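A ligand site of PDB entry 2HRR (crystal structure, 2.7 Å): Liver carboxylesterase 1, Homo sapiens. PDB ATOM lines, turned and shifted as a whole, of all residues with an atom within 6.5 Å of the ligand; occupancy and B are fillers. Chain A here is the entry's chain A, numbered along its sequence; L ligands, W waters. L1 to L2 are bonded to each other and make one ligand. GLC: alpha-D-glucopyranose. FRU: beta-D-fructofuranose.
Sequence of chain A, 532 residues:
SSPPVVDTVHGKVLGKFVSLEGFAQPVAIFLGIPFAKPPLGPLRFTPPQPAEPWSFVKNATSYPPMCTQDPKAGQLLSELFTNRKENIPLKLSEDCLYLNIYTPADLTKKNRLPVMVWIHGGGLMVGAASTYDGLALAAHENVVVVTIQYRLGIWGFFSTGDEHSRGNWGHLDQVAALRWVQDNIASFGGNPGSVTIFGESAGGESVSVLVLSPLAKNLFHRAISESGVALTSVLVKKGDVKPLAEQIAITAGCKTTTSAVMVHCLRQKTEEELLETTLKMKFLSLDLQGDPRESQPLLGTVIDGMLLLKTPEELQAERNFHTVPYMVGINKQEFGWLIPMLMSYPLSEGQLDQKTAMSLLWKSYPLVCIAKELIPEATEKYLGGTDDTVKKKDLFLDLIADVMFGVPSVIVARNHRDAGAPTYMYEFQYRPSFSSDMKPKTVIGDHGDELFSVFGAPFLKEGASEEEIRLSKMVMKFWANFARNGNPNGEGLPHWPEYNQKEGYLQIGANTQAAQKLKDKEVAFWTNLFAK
The backbone carbonyl oxygen (O) of Met 438 lies within hydrogen-bond range of an oxygen (O6) of FRU L2 (3.0 Å). N of Met 341 lies close to O6 of GLC L1 (3.3 Å). O of Gly 336 lies within hydrogen-bond range of O4 of GLC L1 (2.7 Å). The side-chain amino group (NZ) of Lys 393 is in hydrogen-bond range of an oxygen (O3) of GLC L1, 2.8 Å away.
The backbone carbonyl oxygen (O) of Met 438 is in hydrogen-bond range of the indole nitrogen (NE1) of Trp 337 (3.5 Å). The backbone carbonyl oxygen (O) of Pro 340 is in hydrogen-bond range of the backbone NH (N) of Tyr 345 (2.9 Å). NZ of Lys 393 lies within salt-bridge range of OD1 of Asp 394, 3.4 Å away.
O of Leu 347 sits close to O5 of GLC L1 (3.4 Å). Merely in contact with the ligand: Trp 337, Gly 350, Ser 348, Pro 340 and Leu 397. Hydrophobic or aromatic side chains within 4 Å of the ligand: Trp 337, Pro 340, Met 341 and Leu 397. Along chain A the residues within 4 Å of the ligand span positions 336 to 438.
Water W2 bridges an oxygen (O3) of GLC L1 and the backbone carbonyl oxygen of Gly 336.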
ATOM      1  N   PHE A 335     -15.813  -0.208  18.093  1.00  0.00           N
ATOM      2  CA  PHE A 335     -16.805  -1.185  18.538  1.00  0.00           C
ATOM      3  C   PHE A 335     -16.560  -1.539  19.996  1.00  0.00           C
ATOM      4  O   PHE A 335     -16.865  -2.643  20.452  1.00  0.00           O
ATOM      5  CB  PHE A 335     -16.716  -2.448  17.673  1.00  0.00           C
ATOM      6  CG  PHE A 335     -17.995  -3.196  17.540  1.00  0.00           C
ATOM      7  CD1 PHE A 335     -18.188  -4.412  18.202  1.00  0.00           C
ATOM      8  CD2 PHE A 335     -19.021  -2.711  16.728  1.00  0.00           C
ATOM      9  CE1 PHE A 335     -19.373  -5.131  18.050  1.00  0.00           C
ATOM     10  CE2 PHE A 335     -20.210  -3.413  16.570  1.00  0.00           C
ATOM     11  CZ  PHE A 335     -20.389  -4.628  17.231  1.00  0.00           C
ATOM     12  N   GLY A 336     -16.021  -0.574  20.738  1.00  0.00           N
ATOM     13  CA  GLY A 336     -15.709  -0.782  22.136  1.00  0.00           C
ATOM     14  C   GLY A 336     -16.867  -1.062  23.067  1.00  0.00           C
ATOM     15  O   GLY A 336     -16.775  -1.958  23.894  1.00  0.00           O
ATOM     16  N   TRP A 337     -17.973  -0.319  22.959  1.00  0.00           N
ATOM     17  CA  TRP A 337     -19.111  -0.519  23.843  1.00  0.00           C
ATOM     18  C   TRP A 337     -20.478  -0.144  23.245  1.00  0.00           C
ATOM     19  O   TRP A 337     -21.377  -1.014  23.087  1.00  0.00           O
ATOM     20  CB  TRP A 337     -18.937   0.323  25.110  1.00  0.00           C
ATOM     21  CG  TRP A 337     -20.173   0.293  25.975  1.00  0.00           C
ATOM     22  CD1 TRP A 337     -20.601  -0.757  26.722  1.00  0.00           C
ATOM     23  CD2 TRP A 337     -21.141   1.343  26.166  1.00  0.00           C
ATOM     24  NE1 TRP A 337     -21.767  -0.435  27.377  1.00  0.00           N
ATOM     25  CE2 TRP A 337     -22.117   0.845  27.050  1.00  0.00           C
ATOM     26  CE3 TRP A 337     -21.271   2.646  25.666  1.00  0.00           C
ATOM     27  CZ2 TRP A 337     -23.220   1.607  27.465  1.00  0.00           C
ATOM     28  CZ3 TRP A 337     -22.374   3.407  26.081  1.00  0.00           C
ATOM     29  CH2 TRP A 337     -23.332   2.882  26.966  1.00  0.00           C
ATOM     30  N   LEU A 338     -20.645   1.152  22.966  1.00  0.00           N
ATOM     31  CA  LEU A 338     -21.881   1.696  22.449  1.00  0.00           C
ATOM     32  C   LEU A 338     -22.624   0.901  21.404  1.00  0.00           C
ATOM     33  O   LEU A 338     -23.826   0.665  21.542  1.00  0.00           O
ATOM     34  CB  LEU A 338     -21.610   3.081  21.907  1.00  0.00           C
ATOM     35  CG  LEU A 338     -22.765   3.812  21.203  1.00  0.00           C
ATOM     36  CD1 LEU A 338     -23.905   4.079  22.184  1.00  0.00           C
ATOM     37  CD2 LEU A 338     -22.304   5.128  20.606  1.00  0.00           C
ATOM     38  N   ILE A 339     -21.956   0.534  20.326  1.00  0.00           N
ATOM     39  CA  ILE A 339     -22.622  -0.207  19.271  1.00  0.00           C
ATOM     40  C   ILE A 339     -23.060  -1.590  19.735  1.00  0.00           C
ATOM     41  O   ILE A 339     -24.222  -1.943  19.592  1.00  0.00           O
ATOM     42  CB  ILE A 339     -21.732  -0.307  18.014  1.00  0.00           C
ATOM     43  CG1 ILE A 339     -21.387   1.092  17.505  1.00  0.00           C
ATOM     44  CG2 ILE A 339     -22.471  -1.063  16.925  1.00  0.00           C
ATOM     45  CD1 ILE A 339     -20.578   1.097  16.232  1.00  0.00           C
ATOM     46  N   PRO A 340     -22.141  -2.389  20.314  1.00  0.00           N
ATOM     47  CA  PRO A 340     -22.544  -3.724  20.774  1.00  0.00           C
ATOM     48  C   PRO A 340     -23.718  -3.636  21.750  1.00  0.00           C
ATOM     49  O   PRO A 340     -24.681  -4.397  21.659  1.00  0.00           O
ATOM     50  CB  PRO A 340     -21.278  -4.257  21.434  1.00  0.00           C
ATOM     51  CG  PRO A 340     -20.187  -3.594  20.674  1.00  0.00           C
ATOM     52  CD  PRO A 340     -20.694  -2.193  20.503  1.00  0.00           C
ATOM     53  N   MET A 341     -23.608  -2.707  22.694  1.00  0.00           N
ATOM     54  CA  MET A 341     -24.666  -2.508  23.688  1.00  0.00           C
ATOM     55  C   MET A 341     -25.995  -2.218  23.002  1.00  0.00           C
ATOM     56  O   MET A 341     -27.024  -2.807  23.344  1.00  0.00           O
ATOM     57  CB  MET A 341     -24.280  -1.350  24.622  1.00  0.00           C
ATOM     58  CG  MET A 341     -25.359  -0.941  25.616  1.00  0.00           C
ATOM     59  SD  MET A 341     -26.642   0.161  24.924  1.00  0.00           S
ATOM     60  CE  MET A 341     -25.929   1.777  25.270  1.00  0.00           C
ATOM     61  N   LEU A 342     -25.969  -1.310  22.035  1.00  0.00           N
ATOM     62  CA  LEU A 342     -27.170  -0.951  21.304  1.00  0.00           C
ATOM     63  C   LEU A 342     -27.762  -2.130  20.542  1.00  0.00           C
ATOM     64  O   LEU A 342     -28.980  -2.324  20.536  1.00  0.00           O
ATOM     65  CB  LEU A 342     -26.877   0.205  20.333  1.00  0.00           C
ATOM     66  CG  LEU A 342     -26.673   1.581  20.960  1.00  0.00           C
ATOM     67  CD1 LEU A 342     -26.589   2.636  19.863  1.00  0.00           C
ATOM     68  CD2 LEU A 342     -27.833   1.896  21.883  1.00  0.00           C
ATOM     69  N   SER A 344     -27.522  -5.106  21.314  1.00  0.00           N
ATOM     70  CA  SER A 344     -27.713  -6.199  22.253  1.00  0.00           C
ATOM     71  C   SER A 344     -26.836  -7.387  21.868  1.00  0.00           C
ATOM     72  O   SER A 344     -27.335  -8.494  21.658  1.00  0.00           O
ATOM     73  CB  SER A 344     -29.175  -6.638  22.270  1.00  0.00           C
ATOM     74  OG  SER A 344     -30.045  -5.547  22.549  1.00  0.00           O
ATOM     75  N   TYR A 345     -25.533  -7.162  21.784  1.00  0.00           N
ATOM     76  CA  TYR A 345     -24.606  -8.223  21.410  1.00  0.00           C
ATOM     77  C   TYR A 345     -24.496  -9.325  22.457  1.00  0.00           C
ATOM     78  O   TYR A 345     -24.515  -9.067  23.660  1.00  0.00           O
ATOM     79  CB  TYR A 345     -23.216  -7.636  21.148  1.00  0.00           C
ATOM     80  CG  TYR A 345     -22.753  -7.853  19.731  1.00  0.00           C
ATOM     81  CD1 TYR A 345     -23.397  -7.223  18.677  1.00  0.00           C
ATOM     82  CD2 TYR A 345     -21.693  -8.709  19.446  1.00  0.00           C
ATOM     83  CE1 TYR A 345     -23.001  -7.436  17.365  1.00  0.00           C
ATOM     84  CE2 TYR A 345     -21.288  -8.930  18.141  1.00  0.00           C
ATOM     85  CZ  TYR A 345     -21.944  -8.293  17.111  1.00  0.00           C
ATOM     86  OH  TYR A 345     -21.553  -8.516  15.808  1.00  0.00           O
ATOM     87  N   LEU A 347     -22.528 -10.655  24.104  1.00  0.00           N
ATOM     88  CA  LEU A 347     -21.298 -10.567  24.871  1.00  0.00           C
ATOM     89  C   LEU A 347     -21.617 -10.303  26.339  1.00  0.00           C
ATOM     90  O   LEU A 347     -21.006  -9.433  26.965  1.00  0.00           O
ATOM     91  CB  LEU A 347     -20.424  -9.445  24.322  1.00  0.00           C
ATOM     92  CG  LEU A 347     -20.180  -9.464  22.808  1.00  0.00           C
ATOM     93  CD1 LEU A 347     -19.327  -8.265  22.415  1.00  0.00           C
ATOM     94  CD2 LEU A 347     -19.489 -10.771  22.413  1.00  0.00           C
ATOM     95  N   SER A 348     -22.562 -11.059  26.889  1.00  0.00           N
ATOM     96  CA  SER A 348     -22.952 -10.872  28.277  1.00  0.00           C
ATOM     97  C   SER A 348     -21.956 -11.433  29.294  1.00  0.00           C
ATOM     98  O   SER A 348     -21.932 -11.011  30.445  1.00  0.00           O
ATOM     99  CB  SER A 348     -24.325 -11.509  28.515  1.00  0.00           C
ATOM    100  OG  SER A 348     -24.720 -11.377  29.861  1.00  0.00           O
ATOM    101  N   GLU A 349     -21.133 -12.378  28.848  1.00  0.00           N
ATOM    102  CA  GLU A 349     -20.144 -13.020  29.712  1.00  0.00           C
ATOM    103  C   GLU A 349     -18.821 -12.257  29.863  1.00  0.00           C
ATOM    104  O   GLU A 349     -18.133 -12.404  30.877  1.00  0.00           O
ATOM    105  CB  GLU A 349     -19.862 -14.437  29.198  1.00  0.00           C
ATOM    106  CG  GLU A 349     -20.075 -15.560  30.217  1.00  0.00           C
ATOM    107  CD  GLU A 349     -18.901 -15.742  31.169  1.00  0.00           C
ATOM    108  OE1 GLU A 349     -18.975 -16.639  32.042  1.00  0.00           O
ATOM    109  OE2 GLU A 349     -17.896 -15.003  31.041  1.00  0.00           O
ATOM    110  N   GLY A 350     -18.476 -11.447  28.867  1.00  0.00           N
ATOM    111  CA  GLY A 350     -17.224 -10.709  28.940  1.00  0.00           C
ATOM    112  C   GLY A 350     -16.073 -11.686  28.738  1.00  0.00           C
ATOM    113  O   GLY A 350     -14.950 -11.454  29.202  1.00  0.00           O
ATOM    114  N   GLN A 351     -16.381 -12.779  28.046  1.00  0.00           N
ATOM    115  CA  GLN A 351     -15.408 -13.837  27.769  1.00  0.00           C
ATOM    116  C   GLN A 351     -15.781 -14.526  26.453  1.00  0.00           C
ATOM    117  O   GLN A 351     -16.937 -14.877  26.247  1.00  0.00           O
ATOM    118  CB  GLN A 351     -15.428 -14.833  28.922  1.00  0.00           C
ATOM    119  CG  GLN A 351     -14.413 -15.943  28.814  1.00  0.00           C
ATOM    120  CD  GLN A 351     -14.213 -16.670  30.131  1.00  0.00           C
ATOM    121  OE1 GLN A 351     -13.388 -17.574  30.233  1.00  0.00           O
ATOM    122  NE2 GLN A 351     -14.980 -16.268  31.138  1.00  0.00           N
ATOM    123  N   LYS A 393     -12.038 -11.860  23.553  1.00  0.00           N
ATOM    124  CA  LYS A 393     -13.264 -11.067  23.517  1.00  0.00           C
ATOM    125  C   LYS A 393     -12.971  -9.596  23.199  1.00  0.00           C
ATOM    126  O   LYS A 393     -13.812  -8.909  22.603  1.00  0.00           O
ATOM    127  CB  LYS A 393     -13.995 -11.219  24.858  1.00  0.00           C
ATOM    128  CG  LYS A 393     -15.056 -10.183  25.154  1.00  0.00           C
ATOM    129  CD  LYS A 393     -14.449  -9.044  25.936  1.00  0.00           C
ATOM    130  CE  LYS A 393     -15.517  -8.239  26.636  1.00  0.00           C
ATOM    131  NZ  LYS A 393     -14.917  -7.164  27.466  1.00  0.00           N
ATOM    132  N   ASP A 394     -11.798  -9.110  23.579  1.00  0.00           N
ATOM    133  CA  ASP A 394     -11.455  -7.721  23.287  1.00  0.00           C
ATOM    134  C   ASP A 394     -10.900  -7.612  21.868  1.00  0.00           C
ATOM    135  O   ASP A 394     -11.245  -6.690  21.127  1.00  0.00           O
ATOM    136  CB  ASP A 394     -10.430  -7.185  24.292  1.00  0.00           C
ATOM    137  CG  ASP A 394     -11.058  -6.828  25.631  1.00  0.00           C
ATOM    138  OD1 ASP A 394     -12.201  -6.339  25.647  1.00  0.00           O
ATOM    139  OD2 ASP A 394     -10.397  -7.020  26.669  1.00  0.00           O
ATOM    140  N   LEU A 397     -13.603  -7.394  19.424  1.00  0.00           N
ATOM    141  CA  LEU A 397     -14.221  -6.087  19.290  1.00  0.00           C
ATOM    142  C   LEU A 397     -13.366  -5.219  18.364  1.00  0.00           C
ATOM    143  O   LEU A 397     -13.884  -4.355  17.666  1.00  0.00           O
ATOM    144  CB  LEU A 397     -14.350  -5.413  20.657  1.00  0.00           C
ATOM    145  CG  LEU A 397     -15.107  -6.184  21.736  1.00  0.00           C
ATOM    146  CD1 LEU A 397     -15.011  -5.453  23.061  1.00  0.00           C
ATOM    147  CD2 LEU A 397     -16.555  -6.368  21.321  1.00  0.00           C
ATOM    148  N   ASP A 437     -22.529   5.593  32.655  1.00  0.00           N
ATOM    149  CA  ASP A 437     -21.919   4.808  33.730  1.00  0.00           C
ATOM    150  C   ASP A 437     -21.893   3.297  33.483  1.00  0.00           C
ATOM    151  O   ASP A 437     -21.133   2.578  34.146  1.00  0.00           O
ATOM    152  CB  ASP A 437     -22.621   5.111  35.047  1.00  0.00           C
ATOM    153  CG  ASP A 437     -24.123   5.239  34.890  1.00  0.00           C
ATOM    154  OD1 ASP A 437     -24.574   6.288  34.359  1.00  0.00           O
ATOM    155  OD2 ASP A 437     -24.853   4.312  35.306  1.00  0.00           O
ATOM    156  N   MET A 438     -22.696   2.821  32.541  1.00  0.00           N
ATOM    157  CA  MET A 438     -22.755   1.397  32.232  1.00  0.00           C
ATOM    158  C   MET A 438     -21.629   0.985  31.272  1.00  0.00           C
ATOM    159  O   MET A 438     -21.561  -0.165  30.831  1.00  0.00           O
ATOM    160  CB  MET A 438     -24.108   1.059  31.592  1.00  0.00           C
ATOM    161  CG  MET A 438     -25.317   1.378  32.481  1.00  0.00           C
ATOM    162  SD  MET A 438     -26.902   1.223  31.618  1.00  0.00           S
ATOM    163  CE  MET A 438     -27.232   2.966  31.146  1.00  0.00           C
ATOM    164  N   LYS A 439     -20.753   1.938  30.964  1.00  0.00           N
ATOM    165  CA  LYS A 439     -19.639   1.723  30.061  1.00  0.00           C
ATOM    166  C   LYS A 439     -18.373   1.310  30.801  1.00  0.00           C
ATOM    167  O   LYS A 439     -17.873   2.037  31.660  1.00  0.00           O
ATOM    168  CB  LYS A 439     -19.385   3.006  29.270  1.00  0.00           C
ATOM    169  CG  LYS A 439     -18.171   2.995  28.357  1.00  0.00           C
ATOM    170  CD  LYS A 439     -17.971   4.378  27.763  1.00  0.00           C
ATOM    171  CE  LYS A 439     -16.774   4.444  26.850  1.00  0.00           C
ATOM    172  NZ  LYS A 439     -16.644   5.795  26.239  1.00  0.00           N
ATOM    173  N   PRO A 440     -17.833   0.115  30.475  1.00  0.00           N
ATOM    174  CA  PRO A 440     -16.616  -0.378  31.131  1.00  0.00           C
ATOM    175  C   PRO A 440     -15.470   0.630  31.044  1.00  0.00           C
ATOM    176  O   PRO A 440     -15.101   1.082  29.962  1.00  0.00           O
ATOM    177  CB  PRO A 440     -16.323  -1.673  30.364  1.00  0.00           C
ATOM    178  CG  PRO A 440     -16.914  -1.426  29.016  1.00  0.00           C
ATOM    179  CD  PRO A 440     -18.219  -0.766  29.366  1.00  0.00           C
ATOM    180  N   VAL A 443     -12.674   1.072  28.378  1.00  0.00           N
ATOM    181  CA  VAL A 443     -12.966   1.480  27.012  1.00  0.00           C
ATOM    182  C   VAL A 443     -12.707   2.969  26.786  1.00  0.00           C
ATOM    183  O   VAL A 443     -13.388   3.825  27.356  1.00  0.00           O
ATOM    184  CB  VAL A 443     -14.440   1.157  26.643  1.00  0.00           C
ATOM    185  CG1 VAL A 443     -14.778   1.682  25.259  1.00  0.00           C
ATOM    186  CG2 VAL A 443     -14.646  -0.341  26.692  1.00  0.00           C
HETATM  187  C1  GLC L   1     -20.098  -6.680  27.596  1.00  0.00           C
HETATM  188  C2  GLC L   1     -18.615  -6.716  27.165  1.00  0.00           C
HETATM  189  C3  GLC L   1     -18.115  -5.282  26.849  1.00  0.00           C
HETATM  190  C4  GLC L   1     -18.966  -4.711  25.740  1.00  0.00           C
HETATM  191  C5  GLC L   1     -20.443  -4.668  26.171  1.00  0.00           C
HETATM  192  C6  GLC L   1     -21.322  -4.141  25.077  1.00  0.00           C
HETATM  193  O2  GLC L   1     -17.850  -7.339  28.213  1.00  0.00           O
HETATM  194  O3  GLC L   1     -16.753  -5.339  26.453  1.00  0.00           O
HETATM  195  O4  GLC L   1     -18.505  -3.361  25.421  1.00  0.00           O
HETATM  196  O5  GLC L   1     -20.870  -6.035  26.513  1.00  0.00           O
HETATM  197  O6  GLC L   1     -22.696  -4.311  25.412  1.00  0.00           O
HETATM  198  C1  FRU L   2     -21.988  -7.518  29.702  1.00  0.00           C
HETATM  199  C2  FRU L   2     -21.086  -6.301  29.969  1.00  0.00           C
HETATM  200  C3  FRU L   2     -20.134  -6.463  31.188  1.00  0.00           C
HETATM  201  C4  FRU L   2     -20.001  -5.026  31.654  1.00  0.00           C
HETATM  202  C5  FRU L   2     -21.490  -4.662  31.580  1.00  0.00           C
HETATM  203  C6  FRU L   2     -21.915  -3.207  31.730  1.00  0.00           C
HETATM  204  O1  FRU L   2     -23.118  -7.081  28.926  1.00  0.00           O
HETATM  205  O2  FRU L   2     -20.207  -5.904  28.828  1.00  0.00           O
HETATM  206  O3  FRU L   2     -18.891  -7.035  30.837  1.00  0.00           O
HETATM  207  O4  FRU L   2     -19.485  -5.005  32.981  1.00  0.00           O
HETATM  208  O5  FRU L   2     -21.895  -5.189  30.306  1.00  0.00           O
HETATM  209  O6  FRU L   2     -21.128  -2.471  32.651  1.00  0.00           O
HETATM  210  O   HOH W   1     -16.774  -5.151  30.794  1.00  0.00           O
HETATM  211  O   HOH W   2     -15.000  -3.610  25.662  1.00  0.00           O
HETATM  212  O   HOH W   3     -17.249  -5.469  34.496  1.00  0.00           O
